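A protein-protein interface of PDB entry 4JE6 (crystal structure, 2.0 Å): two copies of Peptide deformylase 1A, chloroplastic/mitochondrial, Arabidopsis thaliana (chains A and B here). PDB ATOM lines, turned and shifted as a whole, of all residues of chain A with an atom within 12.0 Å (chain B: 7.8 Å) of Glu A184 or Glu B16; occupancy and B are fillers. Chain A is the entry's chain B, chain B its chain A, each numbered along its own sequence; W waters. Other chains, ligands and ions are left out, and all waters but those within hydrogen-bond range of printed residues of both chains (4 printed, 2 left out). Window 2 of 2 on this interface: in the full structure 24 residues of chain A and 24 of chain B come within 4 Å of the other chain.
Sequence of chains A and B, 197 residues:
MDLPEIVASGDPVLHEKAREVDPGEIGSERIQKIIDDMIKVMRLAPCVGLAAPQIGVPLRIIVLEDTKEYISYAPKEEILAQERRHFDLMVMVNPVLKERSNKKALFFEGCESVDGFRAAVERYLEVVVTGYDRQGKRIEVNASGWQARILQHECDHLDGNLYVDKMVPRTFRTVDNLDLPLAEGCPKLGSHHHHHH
His B15 touches Arg A170 (O to CD, 3.2 Å).
Asp B159 touches Arg A170.
Phe A172 touches His B15.
Asp B11 touches Leu A180.
CB of Ala A183 touches O of His B15, 3.5 Å away.
OE2 of Glu B16 touches CA of Ala A183, at 3.4 Å.
N of Glu A184 sits at hydrogen-bond distance from OE2 of Glu B16.
The backbone carbonyl oxygen of Gly B160 is in hydrogen-bond range of the guanidinium group of Arg A170 (3.2 Å).
The guanidinium group of Arg A170 is in hydrogen-bond range of the side-chain amide oxygen of Asn B161 (2.6 Å).
Water W2 lies within hydrogen-bond range of O of His B15, O of Glu A184 and NH2 of Arg A170.
Water W1 bridges OD1 of Asn B161 (2.7 Å) and NE of Arg A170 (3.4 Å).
Water W3 lies within hydrogen-bond range of the backbone carbonyl oxygen of Asp B159 (2.7 Å) and the guanidinium group of Arg A170 (3.4 Å).
Water W4 lies within hydrogen-bond range of the side-chain amide nitrogen (ND2) of Asn B161 (2.9 Å) and the guanidinium group (NH1) of Arg A170 (3.3 Å).
Pro A169 touches none of the printed residues of chain B.
Printed residues of chain B within 4 Å of Arg A170: His B15, Asp B159, Gly B160 and Asn B161.
Printed residues of chain B within 4 Å of Phe A172: His B15 (3.9 Å).
Printed residues of chain B within 4 Å of Leu A180: Asp B11.
Of chain B, only His B15 (3.5 Å) and Glu B16 (3.4 Å) come within 4 Å of Ala A183.
Of chain B, only Glu B16 (2.8 Å) comes within 4 Å of Glu A184.
Of the printed residues of chain A, Asp B11 touches Leu A180.
Pro B12 touches none of the printed residues of chain A.
His B15 touches three residues of chain A.
Of the printed residues of chain A, Gly B160 touches Arg A170 (3.2 Å).
Printed residues of chain A within 4 Å of Asn B161: Arg A170 (2.6 Å).
The side-chain carboxylate (OD1) of Asp B11 sits at hydrogen-bond distance from the backbone NH (N) of Val B13 (3.0 Å).
O of Asp B11 is in hydrogen-bond range of ND1 of His B15 (3.2 Å).
The backbone carbonyl oxygen (O) of Glu B16 sits close to the backbone NH (N) of Gly B160.
NZ of Lys B17 is in salt-bridge range of OD1 of Asp B159, at 2.8 Å.
NH1 of Arg B60 lies within salt-bridge range of OD1 of Asp B159 (3.1 Å).
The backbone carbonyl oxygen of Ala A183 lies within hydrogen-bond range of the side-chain sulfur of Cys A186, 3.4 Å away.
Hydrophobic or aromatic side chains of chain B within 4 Å of the printed part of chain A: His B15.
Printed residues of chain A that touch a printed residue of chain B: Arg A170, Phe A172, Leu A180, Ala A183 and Glu A184.
Hydrophobic or aromatic side chains of chain A that line the printed part of chain B: Leu A180 and Ala A183.
Among the printed residues, 9 pairs touch across the chains.
No position is printed for both chains.
Of the 9 pairs that touch across the chains among the printed residues, none has its exchanged pair printed and touching as well.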
ATOM      1  N   LEU A 106     -26.622  27.362  -1.951  1.00  0.00           N
ATOM      2  CA  LEU A 106     -25.814  27.326  -0.731  1.00  0.00           C
ATOM      3  C   LEU A 106     -24.329  27.210  -1.096  1.00  0.00           C
ATOM      4  O   LEU A 106     -23.922  26.238  -1.725  1.00  0.00           O
ATOM      5  CB  LEU A 106     -26.253  26.144   0.126  1.00  0.00           C
ATOM      6  CG  LEU A 106     -25.414  25.913   1.377  1.00  0.00           C
ATOM      7  CD1 LEU A 106     -25.616  27.122   2.325  1.00  0.00           C
ATOM      8  CD2 LEU A 106     -25.791  24.573   2.041  1.00  0.00           C
ATOM      9  N   PHE A 108     -20.082  28.681   0.291  1.00  0.00           N
ATOM     10  CA  PHE A 108     -19.238  29.322   1.298  1.00  0.00           C
ATOM     11  C   PHE A 108     -19.039  30.806   1.002  1.00  0.00           C
ATOM     12  O   PHE A 108     -18.810  31.192  -0.157  1.00  0.00           O
ATOM     13  CB  PHE A 108     -17.896  28.589   1.428  1.00  0.00           C
ATOM     14  CG  PHE A 108     -18.000  27.309   2.203  1.00  0.00           C
ATOM     15  CD1 PHE A 108     -18.041  27.335   3.600  1.00  0.00           C
ATOM     16  CD2 PHE A 108     -18.103  26.086   1.548  1.00  0.00           C
ATOM     17  CE1 PHE A 108     -18.163  26.147   4.326  1.00  0.00           C
ATOM     18  CE2 PHE A 108     -18.224  24.899   2.266  1.00  0.00           C
ATOM     19  CZ  PHE A 108     -18.249  24.932   3.650  1.00  0.00           C
ATOM     20  N   VAL A 168     -25.360  28.211   7.830  1.00  0.00           N
ATOM     21  CA  VAL A 168     -25.845  26.842   8.059  1.00  0.00           C
ATOM     22  C   VAL A 168     -25.021  26.258   9.231  1.00  0.00           C
ATOM     23  O   VAL A 168     -23.786  26.369   9.219  1.00  0.00           O
ATOM     24  CB  VAL A 168     -25.648  25.981   6.786  1.00  0.00           C
ATOM     25  CG1 VAL A 168     -25.899  24.484   7.067  1.00  0.00           C
ATOM     26  CG2 VAL A 168     -26.578  26.495   5.639  1.00  0.00           C
ATOM     27  N   PRO A 169     -25.694  25.654  10.243  1.00  0.00           N
ATOM     28  CA  PRO A 169     -24.969  25.095  11.382  1.00  0.00           C
ATOM     29  C   PRO A 169     -23.952  24.042  10.959  1.00  0.00           C
ATOM     30  O   PRO A 169     -24.192  23.286  10.008  1.00  0.00           O
ATOM     31  CB  PRO A 169     -26.069  24.452  12.247  1.00  0.00           C
ATOM     32  CG  PRO A 169     -27.318  25.098  11.821  1.00  0.00           C
ATOM     33  CD  PRO A 169     -27.146  25.466  10.370  1.00  0.00           C
ATOM     34  N   ARG A 170     -22.832  24.008  11.686  1.00  0.00           N
ATOM     35  CA  ARG A 170     -21.756  23.037  11.493  1.00  0.00           C
ATOM     36  C   ARG A 170     -20.949  23.247  10.222  1.00  0.00           C
ATOM     37  O   ARG A 170     -20.221  22.331   9.803  1.00  0.00           O
ATOM     38  CB  ARG A 170     -22.267  21.591  11.580  1.00  0.00           C
ATOM     39  CG  ARG A 170     -22.936  21.330  12.920  1.00  0.00           C
ATOM     40  CD  ARG A 170     -23.287  19.880  13.158  1.00  0.00           C
ATOM     41  NE  ARG A 170     -24.018  19.762  14.412  1.00  0.00           N
ATOM     42  CZ  ARG A 170     -25.049  18.955  14.612  1.00  0.00           C
ATOM     43  NH1 ARG A 170     -25.662  18.949  15.788  1.00  0.00           N
ATOM     44  NH2 ARG A 170     -25.485  18.171  13.630  1.00  0.00           N
ATOM     45  N   THR A 171     -21.024  24.446   9.634  1.00  0.00           N
ATOM     46  CA  THR A 171     -20.229  24.723   8.409  1.00  0.00           C
ATOM     47  C   THR A 171     -19.143  25.776   8.585  1.00  0.00           C
ATOM     48  O   THR A 171     -18.228  25.869   7.759  1.00  0.00           O
ATOM     49  CB  THR A 171     -21.094  25.128   7.195  1.00  0.00           C
ATOM     50  OG1 THR A 171     -21.605  26.462   7.381  1.00  0.00           O
ATOM     51  CG2 THR A 171     -22.236  24.132   6.960  1.00  0.00           C
ATOM     52  N   PHE A 172     -19.233  26.546   9.666  1.00  0.00           N
ATOM     53  CA  PHE A 172     -18.233  27.568   9.984  1.00  0.00           C
ATOM     54  C   PHE A 172     -16.833  26.915  10.035  1.00  0.00           C
ATOM     55  O   PHE A 172     -16.654  25.835  10.599  1.00  0.00           O
ATOM     56  CB  PHE A 172     -18.612  28.249  11.312  1.00  0.00           C
ATOM     57  CG  PHE A 172     -17.729  29.388  11.701  1.00  0.00           C
ATOM     58  CD1 PHE A 172     -16.753  29.216  12.681  1.00  0.00           C
ATOM     59  CD2 PHE A 172     -17.881  30.650  11.107  1.00  0.00           C
ATOM     60  CE1 PHE A 172     -15.935  30.275  13.073  1.00  0.00           C
ATOM     61  CE2 PHE A 172     -17.067  31.722  11.494  1.00  0.00           C
ATOM     62  CZ  PHE A 172     -16.092  31.534  12.491  1.00  0.00           C
ATOM     63  N   ARG A 173     -15.847  27.568   9.428  1.00  0.00           N
ATOM     64  CA  ARG A 173     -14.545  26.939   9.284  1.00  0.00           C
ATOM     65  C   ARG A 173     -13.461  27.945   8.976  1.00  0.00           C
ATOM     66  O   ARG A 173     -13.729  29.045   8.473  1.00  0.00           O
ATOM     67  CB  ARG A 173     -14.594  25.888   8.160  1.00  0.00           C
ATOM     68  CG  ARG A 173     -14.979  26.472   6.769  1.00  0.00           C
ATOM     69  CD  ARG A 173     -15.157  25.349   5.771  1.00  0.00           C
ATOM     70  NE  ARG A 173     -16.072  24.296   6.219  1.00  0.00           N
ATOM     71  CZ  ARG A 173     -16.129  23.070   5.681  1.00  0.00           C
ATOM     72  NH1 ARG A 173     -15.325  22.714   4.667  1.00  0.00           N
ATOM     73  NH2 ARG A 173     -16.998  22.200   6.155  1.00  0.00           N
ATOM     74  N   LEU A 180     -12.406  20.953   3.266  1.00  0.00           N
ATOM     75  CA  LEU A 180     -12.789  19.729   4.000  1.00  0.00           C
ATOM     76  C   LEU A 180     -14.261  19.368   3.781  1.00  0.00           C
ATOM     77  O   LEU A 180     -15.072  20.230   3.415  1.00  0.00           O
ATOM     78  CB  LEU A 180     -12.394  19.816   5.484  1.00  0.00           C
ATOM     79  CG  LEU A 180     -10.896  20.040   5.771  1.00  0.00           C
ATOM     80  CD1 LEU A 180     -10.588  20.041   7.286  1.00  0.00           C
ATOM     81  CD2 LEU A 180     -10.024  18.978   5.062  1.00  0.00           C
ATOM     82  N   PRO A 181     -14.618  18.080   3.944  1.00  0.00           N
ATOM     83  CA  PRO A 181     -16.016  17.720   3.694  1.00  0.00           C
ATOM     84  C   PRO A 181     -16.987  18.446   4.607  1.00  0.00           C
ATOM     85  O   PRO A 181     -16.596  18.971   5.667  1.00  0.00           O
ATOM     86  CB  PRO A 181     -16.054  16.222   3.988  1.00  0.00           C
ATOM     87  CG  PRO A 181     -14.623  15.774   3.806  1.00  0.00           C
ATOM     88  CD  PRO A 181     -13.818  16.905   4.340  1.00  0.00           C
ATOM     89  N   LEU A 182     -18.246  18.486   4.190  1.00  0.00           N
ATOM     90  CA  LEU A 182     -19.327  18.934   5.054  1.00  0.00           C
ATOM     91  C   LEU A 182     -19.675  17.800   5.982  1.00  0.00           C
ATOM     92  O   LEU A 182     -19.620  16.632   5.588  1.00  0.00           O
ATOM     93  CB  LEU A 182     -20.548  19.348   4.236  1.00  0.00           C
ATOM     94  CG  LEU A 182     -20.315  20.485   3.234  1.00  0.00           C
ATOM     95  CD1 LEU A 182     -21.395  20.485   2.156  1.00  0.00           C
ATOM     96  CD2 LEU A 182     -20.275  21.833   3.955  1.00  0.00           C
ATOM     97  N   ALA A 183     -20.028  18.146   7.216  1.00  0.00           N
ATOM     98  CA  ALA A 183     -20.301  17.156   8.255  1.00  0.00           C
ATOM     99  C   ALA A 183     -21.599  16.418   7.980  1.00  0.00           C
ATOM    100  O   ALA A 183     -22.467  16.915   7.252  1.00  0.00           O
ATOM    101  CB  ALA A 183     -20.368  17.830   9.626  1.00  0.00           C
ATOM    102  N   GLU A 184     -21.728  15.236   8.573  1.00  0.00           N
ATOM    103  CA  GLU A 184     -22.987  14.492   8.544  1.00  0.00           C
ATOM    104  C   GLU A 184     -24.179  15.397   8.838  1.00  0.00           C
ATOM    105  O   GLU A 184     -24.159  16.183   9.801  1.00  0.00           O
ATOM    106  CB  GLU A 184     -22.950  13.358   9.542  1.00  0.00           C
ATOM    107  N   GLY A 185     -25.212  15.284   8.013  1.00  0.00           N
ATOM    108  CA  GLY A 185     -26.438  16.054   8.209  1.00  0.00           C
ATOM    109  C   GLY A 185     -26.459  17.451   7.599  1.00  0.00           C
ATOM    110  O   GLY A 185     -27.522  18.068   7.512  1.00  0.00           O
ATOM    111  N   CYS A 186     -25.314  17.971   7.159  1.00  0.00           N
ATOM    112  CA  CYS A 186     -25.324  19.269   6.481  1.00  0.00           C
ATOM    113  C   CYS A 186     -25.919  19.122   5.083  1.00  0.00           C
ATOM    114  O   CYS A 186     -25.675  18.096   4.410  1.00  0.00           O
ATOM    115  CB  CYS A 186     -23.918  19.866   6.366  1.00  0.00           C
ATOM    116  SG  CYS A 186     -23.073  20.151   7.952  1.00  0.00           S
ATOM    117  N   PRO A 187     -26.692  20.138   4.639  1.00  0.00           N
ATOM    118  CA  PRO A 187     -27.165  20.150   3.261  1.00  0.00           C
ATOM    119  C   PRO A 187     -25.973  20.334   2.330  1.00  0.00           C
ATOM    120  O   PRO A 187     -24.961  20.920   2.723  1.00  0.00           O
ATOM    121  CB  PRO A 187     -28.082  21.376   3.193  1.00  0.00           C
ATOM    122  CG  PRO A 187     -27.743  22.206   4.384  1.00  0.00           C
ATOM    123  CD  PRO A 187     -27.153  21.312   5.414  1.00  0.00           C
ATOM    124  N   LYS A 188     -26.104  19.842   1.107  1.00  0.00           N
ATOM    125  CA  LYS A 188     -25.023  19.884   0.139  1.00  0.00           C
ATOM    126  C   LYS A 188     -24.936  21.274  -0.496  1.00  0.00           C
ATOM    127  O   LYS A 188     -25.936  21.974  -0.612  1.00  0.00           O
ATOM    128  CB  LYS A 188     -25.278  18.802  -0.930  1.00  0.00           C
ATOM    129  N   LEU A 189     -23.740  21.678  -0.913  1.00  0.00           N
ATOM    130  CA  LEU A 189     -23.574  22.950  -1.612  1.00  0.00           C
ATOM    131  C   LEU A 189     -24.250  22.905  -2.968  1.00  0.00           C
ATOM    132  O   LEU A 189     -24.471  21.819  -3.523  1.00  0.00           O
ATOM    133  CB  LEU A 189     -22.099  23.306  -1.805  1.00  0.00           C
ATOM    134  CG  LEU A 189     -21.234  23.418  -0.543  1.00  0.00           C
ATOM    135  CD1 LEU A 189     -19.855  23.951  -0.936  1.00  0.00           C
ATOM    136  CD2 LEU A 189     -21.912  24.275   0.531  1.00  0.00           C
ATOM    137  N   ASP B  11     -12.872  20.817  10.359  1.00  0.00           N
ATOM    138  CA  ASP B  11     -12.561  19.389  10.402  1.00  0.00           C
ATOM    139  C   ASP B  11     -13.804  18.676  10.914  1.00  0.00           C
ATOM    140  O   ASP B  11     -14.277  18.989  12.014  1.00  0.00           O
ATOM    141  CB  ASP B  11     -11.353  19.098  11.306  1.00  0.00           C
ATOM    142  CG  ASP B  11     -10.898  17.642  11.227  1.00  0.00           C
ATOM    143  OD1 ASP B  11     -11.742  16.727  11.341  1.00  0.00           O
ATOM    144  OD2 ASP B  11      -9.702  17.408  10.995  1.00  0.00           O
ATOM    145  N   PRO B  12     -14.352  17.728  10.116  1.00  0.00           N
ATOM    146  CA  PRO B  12     -15.621  17.073  10.486  1.00  0.00           C
ATOM    147  C   PRO B  12     -15.647  16.444  11.891  1.00  0.00           C
ATOM    148  O   PRO B  12     -16.724  16.316  12.496  1.00  0.00           O
ATOM    149  CB  PRO B  12     -15.831  16.015   9.387  1.00  0.00           C
ATOM    150  CG  PRO B  12     -14.713  16.172   8.401  1.00  0.00           C
ATOM    151  CD  PRO B  12     -13.805  17.265   8.821  1.00  0.00           C
ATOM    152  N   VAL B  13     -14.490  16.075  12.435  1.00  0.00           N
ATOM    153  CA  VAL B  13     -14.497  15.489  13.801  1.00  0.00           C
ATOM    154  C   VAL B  13     -15.096  16.461  14.843  1.00  0.00           C
ATOM    155  O   VAL B  13     -15.621  16.037  15.879  1.00  0.00           O
ATOM    156  CB  VAL B  13     -13.096  14.962  14.241  1.00  0.00           C
ATOM    157  CG1 VAL B  13     -12.156  16.134  14.533  1.00  0.00           C
ATOM    158  CG2 VAL B  13     -13.229  13.996  15.472  1.00  0.00           C
ATOM    159  N   LEU B  14     -15.027  17.766  14.563  1.00  0.00           N
ATOM    160  CA  LEU B  14     -15.584  18.782  15.464  1.00  0.00           C
ATOM    161  C   LEU B  14     -17.082  18.926  15.324  1.00  0.00           C
ATOM    162  O   LEU B  14     -17.739  19.503  16.187  1.00  0.00           O
ATOM    163  CB  LEU B  14     -14.968  20.144  15.135  1.00  0.00           C
ATOM    164  CG  LEU B  14     -13.828  20.756  15.952  1.00  0.00           C
ATOM    165  CD1 LEU B  14     -13.031  19.840  16.858  1.00  0.00           C
ATOM    166  CD2 LEU B  14     -12.938  21.635  15.112  1.00  0.00           C
ATOM    167  N   HIS B  15     -17.616  18.417  14.220  1.00  0.00           N
ATOM    168  CA  HIS B  15     -18.971  18.770  13.782  1.00  0.00           C
ATOM    169  C   HIS B  15     -19.881  17.548  13.677  1.00  0.00           C
ATOM    170  O   HIS B  15     -20.960  17.628  13.102  1.00  0.00           O
ATOM    171  CB  HIS B  15     -18.891  19.496  12.423  1.00  0.00           C
ATOM    172  CG  HIS B  15     -18.030  20.725  12.456  1.00  0.00           C
ATOM    173  ND1 HIS B  15     -16.831  20.825  11.773  1.00  0.00           N
ATOM    174  CD2 HIS B  15     -18.186  21.897  13.114  1.00  0.00           C
ATOM    175  CE1 HIS B  15     -16.291  22.006  12.009  1.00  0.00           C
ATOM    176  NE2 HIS B  15     -17.101  22.682  12.805  1.00  0.00           N
ATOM    177  N   GLU B  16     -19.421  16.427  14.237  1.00  0.00           N
ATOM    178  CA  GLU B  16     -20.141  15.155  14.225  1.00  0.00           C
ATOM    179  C   GLU B  16     -20.124  14.562  15.624  1.00  0.00           C
ATOM    180  O   GLU B  16     -19.311  14.960  16.467  1.00  0.00           O
ATOM    181  CB  GLU B  16     -19.502  14.197  13.188  1.00  0.00           C
ATOM    182  CG  GLU B  16     -19.741  14.694  11.735  1.00  0.00           C
ATOM    183  CD  GLU B  16     -19.083  13.837  10.660  1.00  0.00           C
ATOM    184  OE1 GLU B  16     -18.306  12.909  10.996  1.00  0.00           O
ATOM    185  OE2 GLU B  16     -19.344  14.104   9.468  1.00  0.00           O
ATOM    186  N   LYS B  17     -21.012  13.612  15.885  1.00  0.00           N
ATOM    187  CA  LYS B  17     -21.194  13.109  17.230  1.00  0.00           C
ATOM    188  C   LYS B  17     -20.116  12.083  17.601  1.00  0.00           C
ATOM    189  O   LYS B  17     -19.960  11.060  16.918  1.00  0.00           O
ATOM    190  CB  LYS B  17     -22.600  12.513  17.373  1.00  0.00           C
ATOM    191  CG  LYS B  17     -22.932  11.969  18.801  1.00  0.00           C
ATOM    192  CD  LYS B  17     -24.358  11.354  18.848  1.00  0.00           C
ATOM    193  CE  LYS B  17     -24.752  10.872  20.268  1.00  0.00           C
ATOM    194  NZ  LYS B  17     -25.391  11.955  21.093  1.00  0.00           N
ATOM    195  N   ALA B  18     -19.385  12.357  18.685  1.00  0.00           N
ATOM    196  CA  ALA B  18     -18.392  11.426  19.208  1.00  0.00           C
ATOM    197  C   ALA B  18     -19.032  10.187  19.873  1.00  0.00           C
ATOM    198  O   ALA B  18     -20.140  10.247  20.381  1.00  0.00           O
ATOM    199  CB  ALA B  18     -17.423  12.130  20.188  1.00  0.00           C
ATOM    200  N   ARG B  19     -18.291   9.082  19.876  1.00  0.00           N
ATOM    201  CA  ARG B  19     -18.770   7.820  20.440  1.00  0.00           C
ATOM    202  C   ARG B  19     -18.349   7.620  21.875  1.00  0.00           C
ATOM    203  O   ARG B  19     -17.288   8.076  22.303  1.00  0.00           O
ATOM    204  CB  ARG B  19     -18.241   6.644  19.628  1.00  0.00           C
ATOM    205  CG  ARG B  19     -18.702   6.683  18.206  1.00  0.00           C
ATOM    206  CD  ARG B  19     -20.208   6.352  17.977  1.00  0.00           C
ATOM    207  NE  ARG B  19     -20.206   6.218  16.531  1.00  0.00           N
ATOM    208  CZ  ARG B  19     -20.201   7.082  15.512  1.00  0.00           C
ATOM    209  NH1 ARG B  19     -19.614   6.667  14.344  1.00  0.00           N
ATOM    210  NH2 ARG B  19     -21.172   8.026  15.455  1.00  0.00           N
ATOM    211  N   PRO B  53     -12.736  15.478  20.651  1.00  0.00           N
ATOM    212  CA  PRO B  53     -12.699  15.819  19.215  1.00  0.00           C
ATOM    213  C   PRO B  53     -11.747  16.973  18.871  1.00  0.00           C
ATOM    214  O   PRO B  53     -11.221  17.020  17.757  1.00  0.00           O
ATOM    215  CB  PRO B  53     -14.157  16.197  18.909  1.00  0.00           C
ATOM    216  CG  PRO B  53     -14.970  15.357  19.899  1.00  0.00           C
ATOM    217  CD  PRO B  53     -14.134  15.456  21.164  1.00  0.00           C
ATOM    218  N   PRO B  58     -12.386  10.837  18.296  1.00  0.00           N
ATOM    219  CA  PRO B  58     -13.857  10.830  18.227  1.00  0.00           C
ATOM    220  C   PRO B  58     -14.509  10.141  19.462  1.00  0.00           C
ATOM    221  O   PRO B  58     -15.345   9.259  19.314  1.00  0.00           O
ATOM    222  CB  PRO B  58     -14.126  10.042  16.940  1.00  0.00           C
ATOM    223  CG  PRO B  58     -12.981   9.034  16.877  1.00  0.00           C
ATOM    224  CD  PRO B  58     -11.775   9.798  17.421  1.00  0.00           C
ATOM    225  N   ARG B  60     -16.136  10.447  23.636  1.00  0.00           N
ATOM    226  CA  ARG B  60     -16.842  11.282  24.589  1.00  0.00           C
ATOM    227  C   ARG B  60     -16.025  11.460  25.882  1.00  0.00           C
ATOM    228  O   ARG B  60     -16.227  10.753  26.869  1.00  0.00           O
ATOM    229  CB  ARG B  60     -18.248  10.729  24.841  1.00  0.00           C
ATOM    230  CG  ARG B  60     -19.071  10.577  23.566  1.00  0.00           C
ATOM    231  CD  ARG B  60     -20.507  10.132  23.865  1.00  0.00           C
ATOM    232  NE  ARG B  60     -21.366  11.244  24.290  1.00  0.00           N
ATOM    233  CZ  ARG B  60     -21.987  12.103  23.468  1.00  0.00           C
ATOM    234  NH1 ARG B  60     -21.837  12.010  22.143  1.00  0.00           N
ATOM    235  NH2 ARG B  60     -22.749  13.080  23.970  1.00  0.00           N
ATOM    236  N   ASP B 156     -21.195  20.032  24.712  1.00  0.00           N
ATOM    237  CA  ASP B 156     -21.618  20.384  23.346  1.00  0.00           C
ATOM    238  C   ASP B 156     -20.666  19.840  22.286  1.00  0.00           C
ATOM    239  O   ASP B 156     -21.128  19.330  21.267  1.00  0.00           O
ATOM    240  CB  ASP B 156     -21.730  21.900  23.157  1.00  0.00           C
ATOM    241  CG  ASP B 156     -23.044  22.475  23.675  1.00  0.00           C
ATOM    242  OD1 ASP B 156     -23.214  23.721  23.587  1.00  0.00           O
ATOM    243  OD2 ASP B 156     -23.892  21.722  24.184  1.00  0.00           O
ATOM    244  N   HIS B 157     -19.350  19.967  22.493  1.00  0.00           N
ATOM    245  CA  HIS B 157     -18.386  19.445  21.493  1.00  0.00           C
ATOM    246  C   HIS B 157     -18.611  17.972  21.133  1.00  0.00           C
ATOM    247  O   HIS B 157     -18.349  17.550  19.993  1.00  0.00           O
ATOM    248  CB  HIS B 157     -16.959  19.565  21.990  1.00  0.00           C
ATOM    249  CG  HIS B 157     -16.345  20.916  21.789  1.00  0.00           C
ATOM    250  ND1 HIS B 157     -16.127  21.461  20.538  1.00  0.00           N
ATOM    251  CD2 HIS B 157     -15.877  21.823  22.682  1.00  0.00           C
ATOM    252  CE1 HIS B 157     -15.558  22.647  20.667  1.00  0.00           C
ATOM    253  NE2 HIS B 157     -15.390  22.892  21.957  1.00  0.00           N
ATOM    254  N   LEU B 158     -19.082  17.196  22.112  1.00  0.00           N
ATOM    255  CA  LEU B 158     -19.207  15.738  21.965  1.00  0.00           C
ATOM    256  C   LEU B 158     -20.374  15.378  21.045  1.00  0.00           C
ATOM    257  O   LEU B 158     -20.411  14.275  20.475  1.00  0.00           O
ATOM    258  CB  LEU B 158     -19.358  15.073  23.346  1.00  0.00           C
ATOM    259  CG  LEU B 158     -18.269  15.356  24.403  1.00  0.00           C
ATOM    260  CD1 LEU B 158     -18.554  14.492  25.667  1.00  0.00           C
ATOM    261  CD2 LEU B 158     -16.850  15.139  23.855  1.00  0.00           C
ATOM    262  N   ASP B 159     -21.303  16.325  20.886  1.00  0.00           N
ATOM    263  CA  ASP B 159     -22.409  16.180  19.931  1.00  0.00           C
ATOM    264  C   ASP B 159     -22.168  16.975  18.647  1.00  0.00           C
ATOM    265  O   ASP B 159     -23.082  17.182  17.846  1.00  0.00           O
ATOM    266  CB  ASP B 159     -23.754  16.506  20.594  1.00  0.00           C
ATOM    267  CG  ASP B 159     -24.207  15.392  21.531  1.00  0.00           C
ATOM    268  OD1 ASP B 159     -23.800  14.225  21.317  1.00  0.00           O
ATOM    269  OD2 ASP B 159     -24.944  15.670  22.485  1.00  0.00           O
ATOM    270  N   GLY B 160     -20.908  17.369  18.439  1.00  0.00           N
ATOM    271  CA  GLY B 160     -20.509  18.062  17.215  1.00  0.00           C
ATOM    272  C   GLY B 160     -21.075  19.476  17.169  1.00  0.00           C
ATOM    273  O   GLY B 160     -21.338  20.007  16.086  1.00  0.00           O
ATOM    274  N   ASN B 161     -21.269  20.082  18.339  1.00  0.00           N
ATOM    275  CA  ASN B 161     -21.815  21.451  18.404  1.00  0.00           C
ATOM    276  C   ASN B 161     -20.823  22.500  18.936  1.00  0.00           C
ATOM    277  O   ASN B 161     -20.231  22.299  19.997  1.00  0.00           O
ATOM    278  CB  ASN B 161     -23.093  21.469  19.251  1.00  0.00           C
ATOM    279  CG  ASN B 161     -24.163  20.554  18.701  1.00  0.00           C
ATOM    280  OD1 ASN B 161     -24.371  20.484  17.486  1.00  0.00           O
ATOM    281  ND2 ASN B 161     -24.837  19.831  19.585  1.00  0.00           N
HETATM  282  O   HOH W   1     -24.729  22.695  15.993  1.00  0.00           O
HETATM  283  O   HOH W   2     -23.020  16.131  12.286  1.00  0.00           O
HETATM  284  O   HOH W   3     -25.406  15.901  17.238  1.00  0.00           O
HETATM  285  O   HOH W   4     -27.003  18.173  18.719  1.00  0.00           O
